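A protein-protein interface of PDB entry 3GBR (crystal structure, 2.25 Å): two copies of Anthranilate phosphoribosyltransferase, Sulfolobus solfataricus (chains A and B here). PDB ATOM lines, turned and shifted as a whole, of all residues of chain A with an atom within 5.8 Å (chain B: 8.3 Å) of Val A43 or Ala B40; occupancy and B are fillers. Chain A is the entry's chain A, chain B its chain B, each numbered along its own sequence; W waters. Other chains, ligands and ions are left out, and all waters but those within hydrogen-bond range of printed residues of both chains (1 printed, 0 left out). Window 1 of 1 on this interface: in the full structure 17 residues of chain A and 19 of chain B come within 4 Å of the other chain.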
ATOM      1  N   ILE A  36     -16.217 -14.874 -13.952  1.00  0.00           N
ATOM      2  CA  ILE A  36     -14.938 -15.080 -14.629  1.00  0.00           C
ATOM      3  C   ILE A  36     -15.149 -15.871 -15.914  1.00  0.00           C
ATOM      4  O   ILE A  36     -14.515 -15.599 -16.930  1.00  0.00           O
ATOM      5  CB  ILE A  36     -13.932 -15.844 -13.709  1.00  0.00           C
ATOM      6  CG1 ILE A  36     -13.368 -14.895 -12.652  1.00  0.00           C
ATOM      7  CG2 ILE A  36     -12.769 -16.436 -14.506  1.00  0.00           C
ATOM      8  CD1 ILE A  36     -12.643 -15.583 -11.521  1.00  0.00           C
ATOM      9  N   VAL A  38     -18.198 -16.204 -17.485  1.00  0.00           N
ATOM     10  CA  VAL A  38     -19.023 -15.367 -18.368  1.00  0.00           C
ATOM     11  C   VAL A  38     -18.144 -14.367 -19.111  1.00  0.00           C
ATOM     12  O   VAL A  38     -18.306 -14.154 -20.303  1.00  0.00           O
ATOM     13  CB  VAL A  38     -20.134 -14.596 -17.605  1.00  0.00           C
ATOM     14  CG1 VAL A  38     -20.880 -13.669 -18.545  1.00  0.00           C
ATOM     15  CG2 VAL A  38     -21.101 -15.555 -16.965  1.00  0.00           C
ATOM     16  N   SER A  39     -17.208 -13.759 -18.392  1.00  0.00           N
ATOM     17  CA  SER A  39     -16.242 -12.841 -18.990  1.00  0.00           C
ATOM     18  C   SER A  39     -15.469 -13.516 -20.137  1.00  0.00           C
ATOM     19  O   SER A  39     -15.369 -12.978 -21.239  1.00  0.00           O
ATOM     20  CB  SER A  39     -15.268 -12.346 -17.915  1.00  0.00           C
ATOM     21  OG  SER A  39     -14.297 -11.478 -18.459  1.00  0.00           O
ATOM     22  N   ALA A  40     -14.939 -14.703 -19.859  1.00  0.00           N
ATOM     23  CA  ALA A  40     -14.171 -15.482 -20.837  1.00  0.00           C
ATOM     24  C   ALA A  40     -14.979 -15.799 -22.092  1.00  0.00           C
ATOM     25  O   ALA A  40     -14.506 -15.599 -23.217  1.00  0.00           O
ATOM     26  CB  ALA A  40     -13.679 -16.772 -20.194  1.00  0.00           C
ATOM     27  N   ILE A  41     -16.196 -16.295 -21.890  1.00  0.00           N
ATOM     28  CA  ILE A  41     -17.073 -16.677 -22.986  1.00  0.00           C
ATOM     29  C   ILE A  41     -17.445 -15.509 -23.895  1.00  0.00           C
ATOM     30  O   ILE A  41     -17.384 -15.631 -25.115  1.00  0.00           O
ATOM     31  CB  ILE A  41     -18.363 -17.327 -22.472  1.00  0.00           C
ATOM     32  CG1 ILE A  41     -18.072 -18.718 -21.901  1.00  0.00           C
ATOM     33  CG2 ILE A  41     -19.399 -17.421 -23.600  1.00  0.00           C
ATOM     34  CD1 ILE A  41     -17.699 -19.745 -22.941  1.00  0.00           C
ATOM     35  N   LEU A  42     -17.828 -14.383 -23.299  1.00  0.00           N
ATOM     36  CA  LEU A  42     -18.161 -13.185 -24.073  1.00  0.00           C
ATOM     37  C   LEU A  42     -16.967 -12.665 -24.857  1.00  0.00           C
ATOM     38  O   LEU A  42     -17.106 -12.175 -25.980  1.00  0.00           O
ATOM     39  CB  LEU A  42     -18.677 -12.067 -23.161  1.00  0.00           C
ATOM     40  CG  LEU A  42     -20.043 -12.242 -22.489  1.00  0.00           C
ATOM     41  CD1 LEU A  42     -20.388 -10.982 -21.698  1.00  0.00           C
ATOM     42  CD2 LEU A  42     -21.150 -12.551 -23.494  1.00  0.00           C
ATOM     43  N   VAL A  43     -15.791 -12.741 -24.252  1.00  0.00           N
ATOM     44  CA  VAL A  43     -14.582 -12.290 -24.918  1.00  0.00           C
ATOM     45  C   VAL A  43     -14.212 -13.258 -26.052  1.00  0.00           C
ATOM     46  O   VAL A  43     -13.851 -12.813 -27.141  1.00  0.00           O
ATOM     47  CB  VAL A  43     -13.435 -12.064 -23.907  1.00  0.00           C
ATOM     48  CG1 VAL A  43     -12.089 -11.951 -24.610  1.00  0.00           C
ATOM     49  CG2 VAL A  43     -13.727 -10.803 -23.073  1.00  0.00           C
ATOM     50  N   ALA A  44     -14.360 -14.564 -25.823  1.00  0.00           N
ATOM     51  CA  ALA A  44     -14.038 -15.560 -26.859  1.00  0.00           C
ATOM     52  C   ALA A  44     -14.985 -15.459 -28.054  1.00  0.00           C
ATOM     53  O   ALA A  44     -14.561 -15.548 -29.208  1.00  0.00           O
ATOM     54  CB  ALA A  44     -14.057 -16.961 -26.284  1.00  0.00           C
ATOM     55  N   LEU A  45     -16.269 -15.284 -27.766  1.00  0.00           N
ATOM     56  CA  LEU A  45     -17.271 -15.021 -28.799  1.00  0.00           C
ATOM     57  C   LEU A  45     -16.872 -13.825 -29.646  1.00  0.00           C
ATOM     58  O   LEU A  45     -16.935 -13.875 -30.879  1.00  0.00           O
ATOM     59  CB  LEU A  45     -18.646 -14.746 -28.175  1.00  0.00           C
ATOM     60  CG  LEU A  45     -19.820 -15.713 -28.364  1.00  0.00           C
ATOM     61  CD1 LEU A  45     -19.425 -17.084 -28.901  1.00  0.00           C
ATOM     62  CD2 LEU A  45     -20.589 -15.819 -27.036  1.00  0.00           C
ATOM     63  N   ARG A  46     -16.469 -12.741 -28.992  1.00  0.00           N
ATOM     64  CA  ARG A  46     -16.062 -11.558 -29.744  1.00  0.00           C
ATOM     65  C   ARG A  46     -14.738 -11.765 -30.485  1.00  0.00           C
ATOM     66  O   ARG A  46     -14.590 -11.284 -31.604  1.00  0.00           O
ATOM     67  CB  ARG A  46     -16.017 -10.298 -28.884  1.00  0.00           C
ATOM     68  CG  ARG A  46     -16.130  -9.049 -29.761  1.00  0.00           C
ATOM     69  CD  ARG A  46     -16.085  -7.750 -28.999  1.00  0.00           C
ATOM     70  NE  ARG A  46     -15.649  -6.662 -29.877  1.00  0.00           N
ATOM     71  CZ  ARG A  46     -15.243  -5.464 -29.469  1.00  0.00           C
ATOM     72  NH1 ARG A  46     -15.218  -5.158 -28.176  1.00  0.00           N
ATOM     73  NH2 ARG A  46     -14.857  -4.561 -30.363  1.00  0.00           N
ATOM     74  N   MET A  47     -13.791 -12.481 -29.869  1.00  0.00           N
ATOM     75  CA  MET A  47     -12.491 -12.771 -30.500  1.00  0.00           C
ATOM     76  C   MET A  47     -12.673 -13.615 -31.755  1.00  0.00           C
ATOM     77  O   MET A  47     -12.100 -13.324 -32.792  1.00  0.00           O
ATOM     78  CB  MET A  47     -11.565 -13.534 -29.548  1.00  0.00           C
ATOM     79  CG  MET A  47     -11.033 -12.746 -28.340  1.00  0.00           C
ATOM     80  SD  MET A  47      -9.774 -11.494 -28.634  1.00  0.00           S
ATOM     81  CE  MET A  47      -8.691 -12.238 -29.867  1.00  0.00           C
ATOM     82  N   LYS A  48     -13.475 -14.670 -31.621  1.00  0.00           N
ATOM     83  CA  LYS A  48     -13.828 -15.567 -32.720  1.00  0.00           C
ATOM     84  C   LYS A  48     -14.626 -14.838 -33.793  1.00  0.00           C
ATOM     85  O   LYS A  48     -14.502 -15.134 -34.984  1.00  0.00           O
ATOM     86  CB  LYS A  48     -14.672 -16.725 -32.182  1.00  0.00           C
ATOM     87  CG  LYS A  48     -15.070 -17.761 -33.221  1.00  0.00           C
ATOM     88  CD  LYS A  48     -15.931 -18.869 -32.620  1.00  0.00           C
ATOM     89  CE  LYS A  48     -17.335 -18.383 -32.252  1.00  0.00           C
ATOM     90  NZ  LYS A  48     -18.048 -17.734 -33.388  1.00  0.00           N
ATOM     91  N   LEU A 167     -16.450  -5.357 -17.905  1.00  0.00           N
ATOM     92  CA  LEU A 167     -15.716  -5.581 -19.163  1.00  0.00           C
ATOM     93  C   LEU A 167     -15.449  -4.267 -19.893  1.00  0.00           C
ATOM     94  O   LEU A 167     -14.347  -4.040 -20.394  1.00  0.00           O
ATOM     95  CB  LEU A 167     -16.474  -6.549 -20.087  1.00  0.00           C
ATOM     96  CG  LEU A 167     -16.125  -8.035 -19.968  1.00  0.00           C
ATOM     97  CD1 LEU A 167     -17.145  -8.887 -20.700  1.00  0.00           C
ATOM     98  CD2 LEU A 167     -14.715  -8.302 -20.498  1.00  0.00           C
ATOM     99  N   ILE A 169     -16.439  -3.249 -22.731  1.00  0.00           N
ATOM    100  CA  ILE A 169     -16.349  -3.400 -24.179  1.00  0.00           C
ATOM    101  C   ILE A 169     -17.690  -3.925 -24.669  1.00  0.00           C
ATOM    102  O   ILE A 169     -18.464  -4.508 -23.894  1.00  0.00           O
ATOM    103  CB  ILE A 169     -15.224  -4.384 -24.615  1.00  0.00           C
ATOM    104  CG1 ILE A 169     -15.409  -5.762 -23.965  1.00  0.00           C
ATOM    105  CG2 ILE A 169     -13.851  -3.821 -24.277  1.00  0.00           C
ATOM    106  CD1 ILE A 169     -14.573  -6.848 -24.593  1.00  0.00           C
ATOM    107  N   ILE B   3      -6.109  -0.564 -18.527  1.00  0.00           N
ATOM    108  CA  ILE B   3      -6.591  -1.932 -18.740  1.00  0.00           C
ATOM    109  C   ILE B   3      -7.662  -2.019 -19.829  1.00  0.00           C
ATOM    110  O   ILE B   3      -7.756  -3.014 -20.551  1.00  0.00           O
ATOM    111  CB  ILE B   3      -7.168  -2.532 -17.427  1.00  0.00           C
ATOM    112  CG1 ILE B   3      -6.146  -2.453 -16.285  1.00  0.00           C
ATOM    113  CG2 ILE B   3      -7.605  -3.980 -17.633  1.00  0.00           C
ATOM    114  CD1 ILE B   3      -4.737  -2.899 -16.660  1.00  0.00           C
ATOM    115  N   ILE B   6      -6.081  -1.510 -23.526  1.00  0.00           N
ATOM    116  CA  ILE B   6      -5.318  -2.749 -23.731  1.00  0.00           C
ATOM    117  C   ILE B   6      -6.231  -3.886 -24.197  1.00  0.00           C
ATOM    118  O   ILE B   6      -5.929  -4.585 -25.172  1.00  0.00           O
ATOM    119  CB  ILE B   6      -4.597  -3.177 -22.430  1.00  0.00           C
ATOM    120  CG1 ILE B   6      -3.292  -2.396 -22.252  1.00  0.00           C
ATOM    121  CG2 ILE B   6      -4.302  -4.676 -22.429  1.00  0.00           C
ATOM    122  CD1 ILE B   6      -2.186  -2.799 -23.222  1.00  0.00           C
ATOM    123  N   LEU B   7      -7.350  -4.065 -23.495  1.00  0.00           N
ATOM    124  CA  LEU B   7      -8.310  -5.112 -23.835  1.00  0.00           C
ATOM    125  C   LEU B   7      -8.884  -4.910 -25.240  1.00  0.00           C
ATOM    126  O   LEU B   7      -8.932  -5.854 -26.035  1.00  0.00           O
ATOM    127  CB  LEU B   7      -9.432  -5.168 -22.794  1.00  0.00           C
ATOM    128  CG  LEU B   7     -10.407  -6.351 -22.852  1.00  0.00           C
ATOM    129  CD1 LEU B   7      -9.692  -7.674 -23.110  1.00  0.00           C
ATOM    130  CD2 LEU B   7     -11.218  -6.428 -21.554  1.00  0.00           C
ATOM    131  N   LEU B  10      -6.243  -5.802 -27.619  1.00  0.00           N
ATOM    132  CA  LEU B  10      -6.115  -7.263 -27.700  1.00  0.00           C
ATOM    133  C   LEU B  10      -7.264  -7.862 -28.493  1.00  0.00           C
ATOM    134  O   LEU B  10      -7.055  -8.749 -29.319  1.00  0.00           O
ATOM    135  CB  LEU B  10      -6.065  -7.896 -26.305  1.00  0.00           C
ATOM    136  CG  LEU B  10      -4.741  -7.830 -25.540  1.00  0.00           C
ATOM    137  CD1 LEU B  10      -4.854  -8.591 -24.212  1.00  0.00           C
ATOM    138  CD2 LEU B  10      -3.588  -8.378 -26.378  1.00  0.00           C
ATOM    139  N   ILE B  11      -8.473  -7.359 -28.247  1.00  0.00           N
ATOM    140  CA  ILE B  11      -9.670  -7.809 -28.965  1.00  0.00           C
ATOM    141  C   ILE B  11      -9.539  -7.577 -30.473  1.00  0.00           C
ATOM    142  O   ILE B  11      -9.977  -8.405 -31.274  1.00  0.00           O
ATOM    143  CB  ILE B  11     -10.945  -7.108 -28.432  1.00  0.00           C
ATOM    144  CG1 ILE B  11     -11.322  -7.658 -27.049  1.00  0.00           C
ATOM    145  CG2 ILE B  11     -12.109  -7.281 -29.406  1.00  0.00           C
ATOM    146  CD1 ILE B  11     -11.869  -9.066 -27.069  1.00  0.00           C
ATOM    147  N   LYS B  13      -6.841  -7.771 -32.026  1.00  0.00           N
ATOM    148  CA  LYS B  13      -5.738  -8.659 -32.437  1.00  0.00           C
ATOM    149  C   LYS B  13      -4.453  -7.891 -32.779  1.00  0.00           C
ATOM    150  O   LYS B  13      -3.662  -8.302 -33.633  1.00  0.00           O
ATOM    151  CB  LYS B  13      -6.185  -9.598 -33.564  1.00  0.00           C
ATOM    152  CG  LYS B  13      -7.336 -10.490 -33.128  1.00  0.00           C
ATOM    153  CD  LYS B  13      -8.104 -11.080 -34.276  1.00  0.00           C
ATOM    154  CE  LYS B  13      -9.293 -11.880 -33.744  1.00  0.00           C
ATOM    155  NZ  LYS B  13     -10.100 -12.511 -34.828  1.00  0.00           N
ATOM    156  N   ILE B  28      -1.797  -6.777 -13.191  1.00  0.00           N
ATOM    157  CA  ILE B  28      -2.476  -8.055 -12.940  1.00  0.00           C
ATOM    158  C   ILE B  28      -1.891  -8.788 -11.740  1.00  0.00           C
ATOM    159  O   ILE B  28      -2.625  -9.181 -10.818  1.00  0.00           O
ATOM    160  CB  ILE B  28      -2.393  -8.991 -14.165  1.00  0.00           C
ATOM    161  CG1 ILE B  28      -3.307  -8.486 -15.285  1.00  0.00           C
ATOM    162  CG2 ILE B  28      -2.793 -10.422 -13.775  1.00  0.00           C
ATOM    163  CD1 ILE B  28      -3.099  -9.197 -16.606  1.00  0.00           C
ATOM    164  N   VAL B  33      -6.082  -5.360 -10.950  1.00  0.00           N
ATOM    165  CA  VAL B  33      -7.039  -5.530 -12.046  1.00  0.00           C
ATOM    166  C   VAL B  33      -8.163  -6.489 -11.634  1.00  0.00           C
ATOM    167  O   VAL B  33      -7.887  -7.581 -11.141  1.00  0.00           O
ATOM    168  CB  VAL B  33      -6.329  -6.037 -13.312  1.00  0.00           C
ATOM    169  CG1 VAL B  33      -7.326  -6.266 -14.452  1.00  0.00           C
ATOM    170  CG2 VAL B  33      -5.260  -5.041 -13.737  1.00  0.00           C
ATOM    171  N   PRO B  34      -9.436  -6.080 -11.817  1.00  0.00           N
ATOM    172  CA  PRO B  34     -10.555  -6.940 -11.427  1.00  0.00           C
ATOM    173  C   PRO B  34     -10.526  -8.310 -12.103  1.00  0.00           C
ATOM    174  O   PRO B  34     -10.045  -8.443 -13.233  1.00  0.00           O
ATOM    175  CB  PRO B  34     -11.789  -6.144 -11.871  1.00  0.00           C
ATOM    176  CG  PRO B  34     -11.333  -4.741 -11.924  1.00  0.00           C
ATOM    177  CD  PRO B  34      -9.910  -4.796 -12.366  1.00  0.00           C
ATOM    178  N   GLU B  35     -11.040  -9.315 -11.410  1.00  0.00           N
ATOM    179  CA  GLU B  35     -10.927 -10.689 -11.887  1.00  0.00           C
ATOM    180  C   GLU B  35     -11.566 -10.863 -13.272  1.00  0.00           C
ATOM    181  O   GLU B  35     -11.038 -11.584 -14.117  1.00  0.00           O
ATOM    182  CB  GLU B  35     -11.533 -11.658 -10.878  1.00  0.00           C
ATOM    183  CG  GLU B  35     -10.739 -11.797  -9.590  1.00  0.00           C
ATOM    184  CD  GLU B  35     -11.180 -12.987  -8.770  1.00  0.00           C
ATOM    185  OE1 GLU B  35     -12.381 -13.323  -8.818  1.00  0.00           O
ATOM    186  OE2 GLU B  35     -10.330 -13.592  -8.078  1.00  0.00           O
ATOM    187  N   ILE B  36     -12.670 -10.154 -13.499  1.00  0.00           N
ATOM    188  CA  ILE B  36     -13.408 -10.193 -14.754  1.00  0.00           C
ATOM    189  C   ILE B  36     -12.530  -9.739 -15.915  1.00  0.00           C
ATOM    190  O   ILE B  36     -12.574 -10.324 -16.995  1.00  0.00           O
ATOM    191  CB  ILE B  36     -14.672  -9.277 -14.678  1.00  0.00           C
ATOM    192  CG1 ILE B  36     -15.799  -9.979 -13.924  1.00  0.00           C
ATOM    193  CG2 ILE B  36     -15.167  -8.885 -16.065  1.00  0.00           C
ATOM    194  CD1 ILE B  36     -16.919  -9.033 -13.464  1.00  0.00           C
ATOM    195  N   LEU B  37     -11.748  -8.686 -15.685  1.00  0.00           N
ATOM    196  CA  LEU B  37     -10.865  -8.139 -16.713  1.00  0.00           C
ATOM    197  C   LEU B  37      -9.605  -8.980 -16.887  1.00  0.00           C
ATOM    198  O   LEU B  37      -9.097  -9.114 -18.009  1.00  0.00           O
ATOM    199  CB  LEU B  37     -10.503  -6.684 -16.396  1.00  0.00           C
ATOM    200  CG  LEU B  37     -11.601  -5.682 -16.744  1.00  0.00           C
ATOM    201  CD1 LEU B  37     -11.348  -4.334 -16.074  1.00  0.00           C
ATOM    202  CD2 LEU B  37     -11.740  -5.537 -18.257  1.00  0.00           C
ATOM    203  N   VAL B  38      -9.104  -9.545 -15.789  1.00  0.00           N
ATOM    204  CA  VAL B  38      -7.968 -10.469 -15.847  1.00  0.00           C
ATOM    205  C   VAL B  38      -8.339 -11.675 -16.729  1.00  0.00           C
ATOM    206  O   VAL B  38      -7.597 -12.041 -17.644  1.00  0.00           O
ATOM    207  CB  VAL B  38      -7.493 -10.897 -14.424  1.00  0.00           C
ATOM    208  CG1 VAL B  38      -6.451 -12.019 -14.488  1.00  0.00           C
ATOM    209  CG2 VAL B  38      -6.901  -9.709 -13.686  1.00  0.00           C
ATOM    210  N   SER B  39      -9.502 -12.264 -16.471  1.00  0.00           N
ATOM    211  CA  SER B  39     -10.006 -13.366 -17.289  1.00  0.00           C
ATOM    212  C   SER B  39     -10.111 -12.962 -18.757  1.00  0.00           C
ATOM    213  O   SER B  39      -9.682 -13.700 -19.651  1.00  0.00           O
ATOM    214  CB  SER B  39     -11.373 -13.817 -16.790  1.00  0.00           C
ATOM    215  OG  SER B  39     -11.950 -14.766 -17.674  1.00  0.00           O
ATOM    216  N   ALA B  40     -10.693 -11.789 -18.998  1.00  0.00           N
ATOM    217  CA  ALA B  40     -10.794 -11.240 -20.350  1.00  0.00           C
ATOM    218  C   ALA B  40      -9.425 -11.111 -21.031  1.00  0.00           C
ATOM    219  O   ALA B  40      -9.254 -11.516 -22.183  1.00  0.00           O
ATOM    220  CB  ALA B  40     -11.487  -9.887 -20.314  1.00  0.00           C
ATOM    221  N   ILE B  41      -8.464 -10.523 -20.322  1.00  0.00           N
ATOM    222  CA  ILE B  41      -7.116 -10.330 -20.860  1.00  0.00           C
ATOM    223  C   ILE B  41      -6.432 -11.666 -21.162  1.00  0.00           C
ATOM    224  O   ILE B  41      -5.889 -11.872 -22.250  1.00  0.00           O
ATOM    225  CB  ILE B  41      -6.239  -9.519 -19.893  1.00  0.00           C
ATOM    226  CG1 ILE B  41      -6.640  -8.039 -19.925  1.00  0.00           C
ATOM    227  CG2 ILE B  41      -4.761  -9.663 -20.253  1.00  0.00           C
ATOM    228  CD1 ILE B  41      -6.074  -7.282 -21.115  1.00  0.00           C
ATOM    229  N   LEU B  42      -6.479 -12.581 -20.206  1.00  0.00           N
ATOM    230  CA  LEU B  42      -5.814 -13.875 -20.379  1.00  0.00           C
ATOM    231  C   LEU B  42      -6.396 -14.682 -21.542  1.00  0.00           C
ATOM    232  O   LEU B  42      -5.650 -15.326 -22.286  1.00  0.00           O
ATOM    233  CB  LEU B  42      -5.837 -14.674 -19.076  1.00  0.00           C
ATOM    234  CG  LEU B  42      -4.911 -14.148 -17.972  1.00  0.00           C
ATOM    235  CD1 LEU B  42      -4.884 -15.125 -16.811  1.00  0.00           C
ATOM    236  CD2 LEU B  42      -3.483 -13.902 -18.469  1.00  0.00           C
ATOM    237  N   VAL B  43      -7.716 -14.621 -21.715  1.00  0.00           N
ATOM    238  CA  VAL B  43      -8.382 -15.261 -22.855  1.00  0.00           C
ATOM    239  C   VAL B  43      -8.066 -14.571 -24.192  1.00  0.00           C
ATOM    240  O   VAL B  43      -7.839 -15.239 -25.206  1.00  0.00           O
ATOM    241  CB  VAL B  43      -9.917 -15.319 -22.653  1.00  0.00           C
ATOM    242  CG1 VAL B  43     -10.637 -15.736 -23.949  1.00  0.00           C
ATOM    243  CG2 VAL B  43     -10.259 -16.276 -21.521  1.00  0.00           C
ATOM    244  N   ALA B  44      -8.061 -13.243 -24.191  1.00  0.00           N
ATOM    245  CA  ALA B  44      -7.786 -12.469 -25.406  1.00  0.00           C
ATOM    246  C   ALA B  44      -6.366 -12.716 -25.916  1.00  0.00           C
ATOM    247  O   ALA B  44      -6.142 -12.867 -27.120  1.00  0.00           O
ATOM    248  CB  ALA B  44      -8.004 -10.986 -25.151  1.00  0.00           C
ATOM    249  N   LEU B  45      -5.415 -12.731 -24.985  1.00  0.00           N
ATOM    250  CA  LEU B  45      -4.015 -13.060 -25.285  1.00  0.00           C
ATOM    251  C   LEU B  45      -3.899 -14.426 -25.966  1.00  0.00           C
ATOM    252  O   LEU B  45      -3.228 -14.567 -26.992  1.00  0.00           O
ATOM    253  CB  LEU B  45      -3.182 -13.047 -23.991  1.00  0.00           C
ATOM    254  CG  LEU B  45      -2.101 -11.989 -23.706  1.00  0.00           C
ATOM    255  CD1 LEU B  45      -1.987 -10.866 -24.736  1.00  0.00           C
ATOM    256  CD2 LEU B  45      -2.291 -11.433 -22.297  1.00  0.00           C
ATOM    257  N   ARG B  46      -4.564 -15.426 -25.393  1.00  0.00           N
ATOM    258  CA  ARG B  46      -4.514 -16.781 -25.937  1.00  0.00           C
ATOM    259  C   ARG B  46      -5.184 -16.910 -27.307  1.00  0.00           C
ATOM    260  O   ARG B  46      -4.667 -17.592 -28.193  1.00  0.00           O
ATOM    261  CB  ARG B  46      -5.135 -17.794 -24.979  1.00  0.00           C
ATOM    262  CG  ARG B  46      -5.263 -19.156 -25.631  1.00  0.00           C
ATOM    263  CD  ARG B  46      -5.357 -20.298 -24.685  1.00  0.00           C
ATOM    264  NE  ARG B  46      -5.448 -21.544 -25.449  1.00  0.00           N
ATOM    265  CZ  ARG B  46      -5.706 -22.738 -24.929  1.00  0.00           C
ATOM    266  NH1 ARG B  46      -5.900 -22.876 -23.622  1.00  0.00           N
ATOM    267  NH2 ARG B  46      -5.770 -23.801 -25.723  1.00  0.00           N
ATOM    268  N   MET B  47      -6.338 -16.274 -27.481  1.00  0.00           N
ATOM    269  CA  MET B  47      -7.041 -16.362 -28.755  1.00  0.00           C
ATOM    270  C   MET B  47      -6.348 -15.567 -29.865  1.00  0.00           C
ATOM    271  O   MET B  47      -6.305 -16.021 -31.004  1.00  0.00           O
ATOM    272  CB  MET B  47      -8.491 -15.936 -28.586  1.00  0.00           C
ATOM    273  CG  MET B  47      -9.262 -16.937 -27.760  1.00  0.00           C
ATOM    274  SD  MET B  47     -11.020 -16.818 -27.960  1.00  0.00           S
ATOM    275  CE  MET B  47     -11.236 -17.022 -29.724  1.00  0.00           C
ATOM    276  N   VAL B 163      -8.480 -16.717 -10.750  1.00  0.00           N
ATOM    277  CA  VAL B 163      -8.882 -16.576 -12.150  1.00  0.00           C
ATOM    278  C   VAL B 163      -8.339 -17.744 -12.951  1.00  0.00           C
ATOM    279  O   VAL B 163      -9.067 -18.379 -13.704  1.00  0.00           O
ATOM    280  CB  VAL B 163      -8.374 -15.259 -12.776  1.00  0.00           C
ATOM    281  CG1 VAL B 163      -8.431 -15.325 -14.298  1.00  0.00           C
ATOM    282  CG2 VAL B 163      -9.184 -14.073 -12.258  1.00  0.00           C
ATOM    283  N   LEU B 167     -10.738 -20.448 -14.670  1.00  0.00           N
ATOM    284  CA  LEU B 167     -10.693 -20.537 -16.136  1.00  0.00           C
ATOM    285  C   LEU B 167     -10.459 -21.962 -16.633  1.00  0.00           C
ATOM    286  O   LEU B 167     -11.003 -22.361 -17.660  1.00  0.00           O
ATOM    287  CB  LEU B 167      -9.597 -19.630 -16.713  1.00  0.00           C
ATOM    288  CG  LEU B 167      -9.954 -18.179 -17.027  1.00  0.00           C
ATOM    289  CD1 LEU B 167      -8.716 -17.463 -17.540  1.00  0.00           C
ATOM    290  CD2 LEU B 167     -11.084 -18.096 -18.048  1.00  0.00           C
HETATM  291  O   HOH W   1     -12.898 -12.562 -35.856  1.00  0.00           O
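Among the printed residues, pairs that only touch across the chains: Ala A44 with Met B47 (3.5 Å), Met A47 with Met B47 (3.5 Å), Ile A36 with Glu B35 (3.5 Å), Met A47 with Ile B11 (3.6 Å), Leu A167 with Ala B40 (3.6 Å), Ala A40 with Leu B167 (3.6 Å), Arg A46 with Ile B11 (3.6 Å), Ala A40 with Ser B39 (3.7 Å), Ser A39 with Ala B40 (3.7 Å), Val A43 with Ala B40 (3.7 Å), Leu A167 with Leu B37 (3.7 Å), Ala A40 with Val B43 (3.7 Å), Lys A48 with Met B47 (3.8 Å), Val A43 with Ile B11 (3.8 Å), Met A47 with Ala B44 (3.8 Å), Ile A36 with Val B163 (3.8 Å) and Met A47 with Leu B10 (3.9 Å).
Water W1 lies within hydrogen-bond range of the side-chain amino group of Lys B13 (3.0 Å), the backbone carbonyl oxygen of Lys A48 (3.2 Å) and the backbone carbonyl oxygen of Met A47 (3.3 Å).
Ile A36 touches Ser B39, and with the chains exchanged Ser A39 touches Ile B36. Ser A39 touches Ala B40, and with the chains exchanged Ala A40 touches Ser B39. Ala A44 touches Met B47, and with the chains exchanged Met A47 touches Ala B44. Met A47 touches its own counterpart, Met B47.
Hydrophobic or aromatic side chains of chain B within 4 Å of the printed part of chain A: Ile B11, Ile B36, Leu B37, Ala B40, Val B43, Ala B44, Met B47, Val B163 and Leu B167. Along chain B the printed residues that touch a printed residue of chain A span positions 10 to 167. Printed residues of chain A that touch a printed residue of chain B: Ile A36, Ser A39, Ala A40, Val A43, Ala A44, Arg A46, Met A47, Lys A48 and Leu A167. Among the printed residues, 20 pairs touch across the chains. Among the printed residues, no Asp or Glu carboxylate lies within 4 Å of a Lys or Arg side-chain nitrogen of the other chain.
Of the printed residues of chain B, Val A43 touches Ile B11 and Ala B40. Ala B40 touches three residues of chain A. Of chain B, only Met B47 (3.5 Å) comes within 4 Å of Ala A44. Of the printed residues of chain A, Leu B167 touches Ala A40 (3.6 Å). Printed residues of chain A within 4 Å of Leu B37: Leu A167. Printed residues of chain A within 4 Å of Ala B44: Met A47 (3.8 Å). Ile B6 touches none of the printed residues of chain A. The nearest residue of chain A that does not touch Ala B40 is Ala A40 (5.2 Å).
The backbone carbonyl oxygen of Ile A36 is in hydrogen-bond range of the side-chain hydroxyl of Ser B39, at 2.8 Å. The side-chain hydroxyl (OG) of Ser A39 is in hydrogen-bond range of the backbone carbonyl oxygen (O) of Ile B36, 2.5 Å away. The backbone carbonyl oxygen (O) of Met A47 is in hydrogen-bond range of the side-chain amino group (NZ) of Lys B13.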
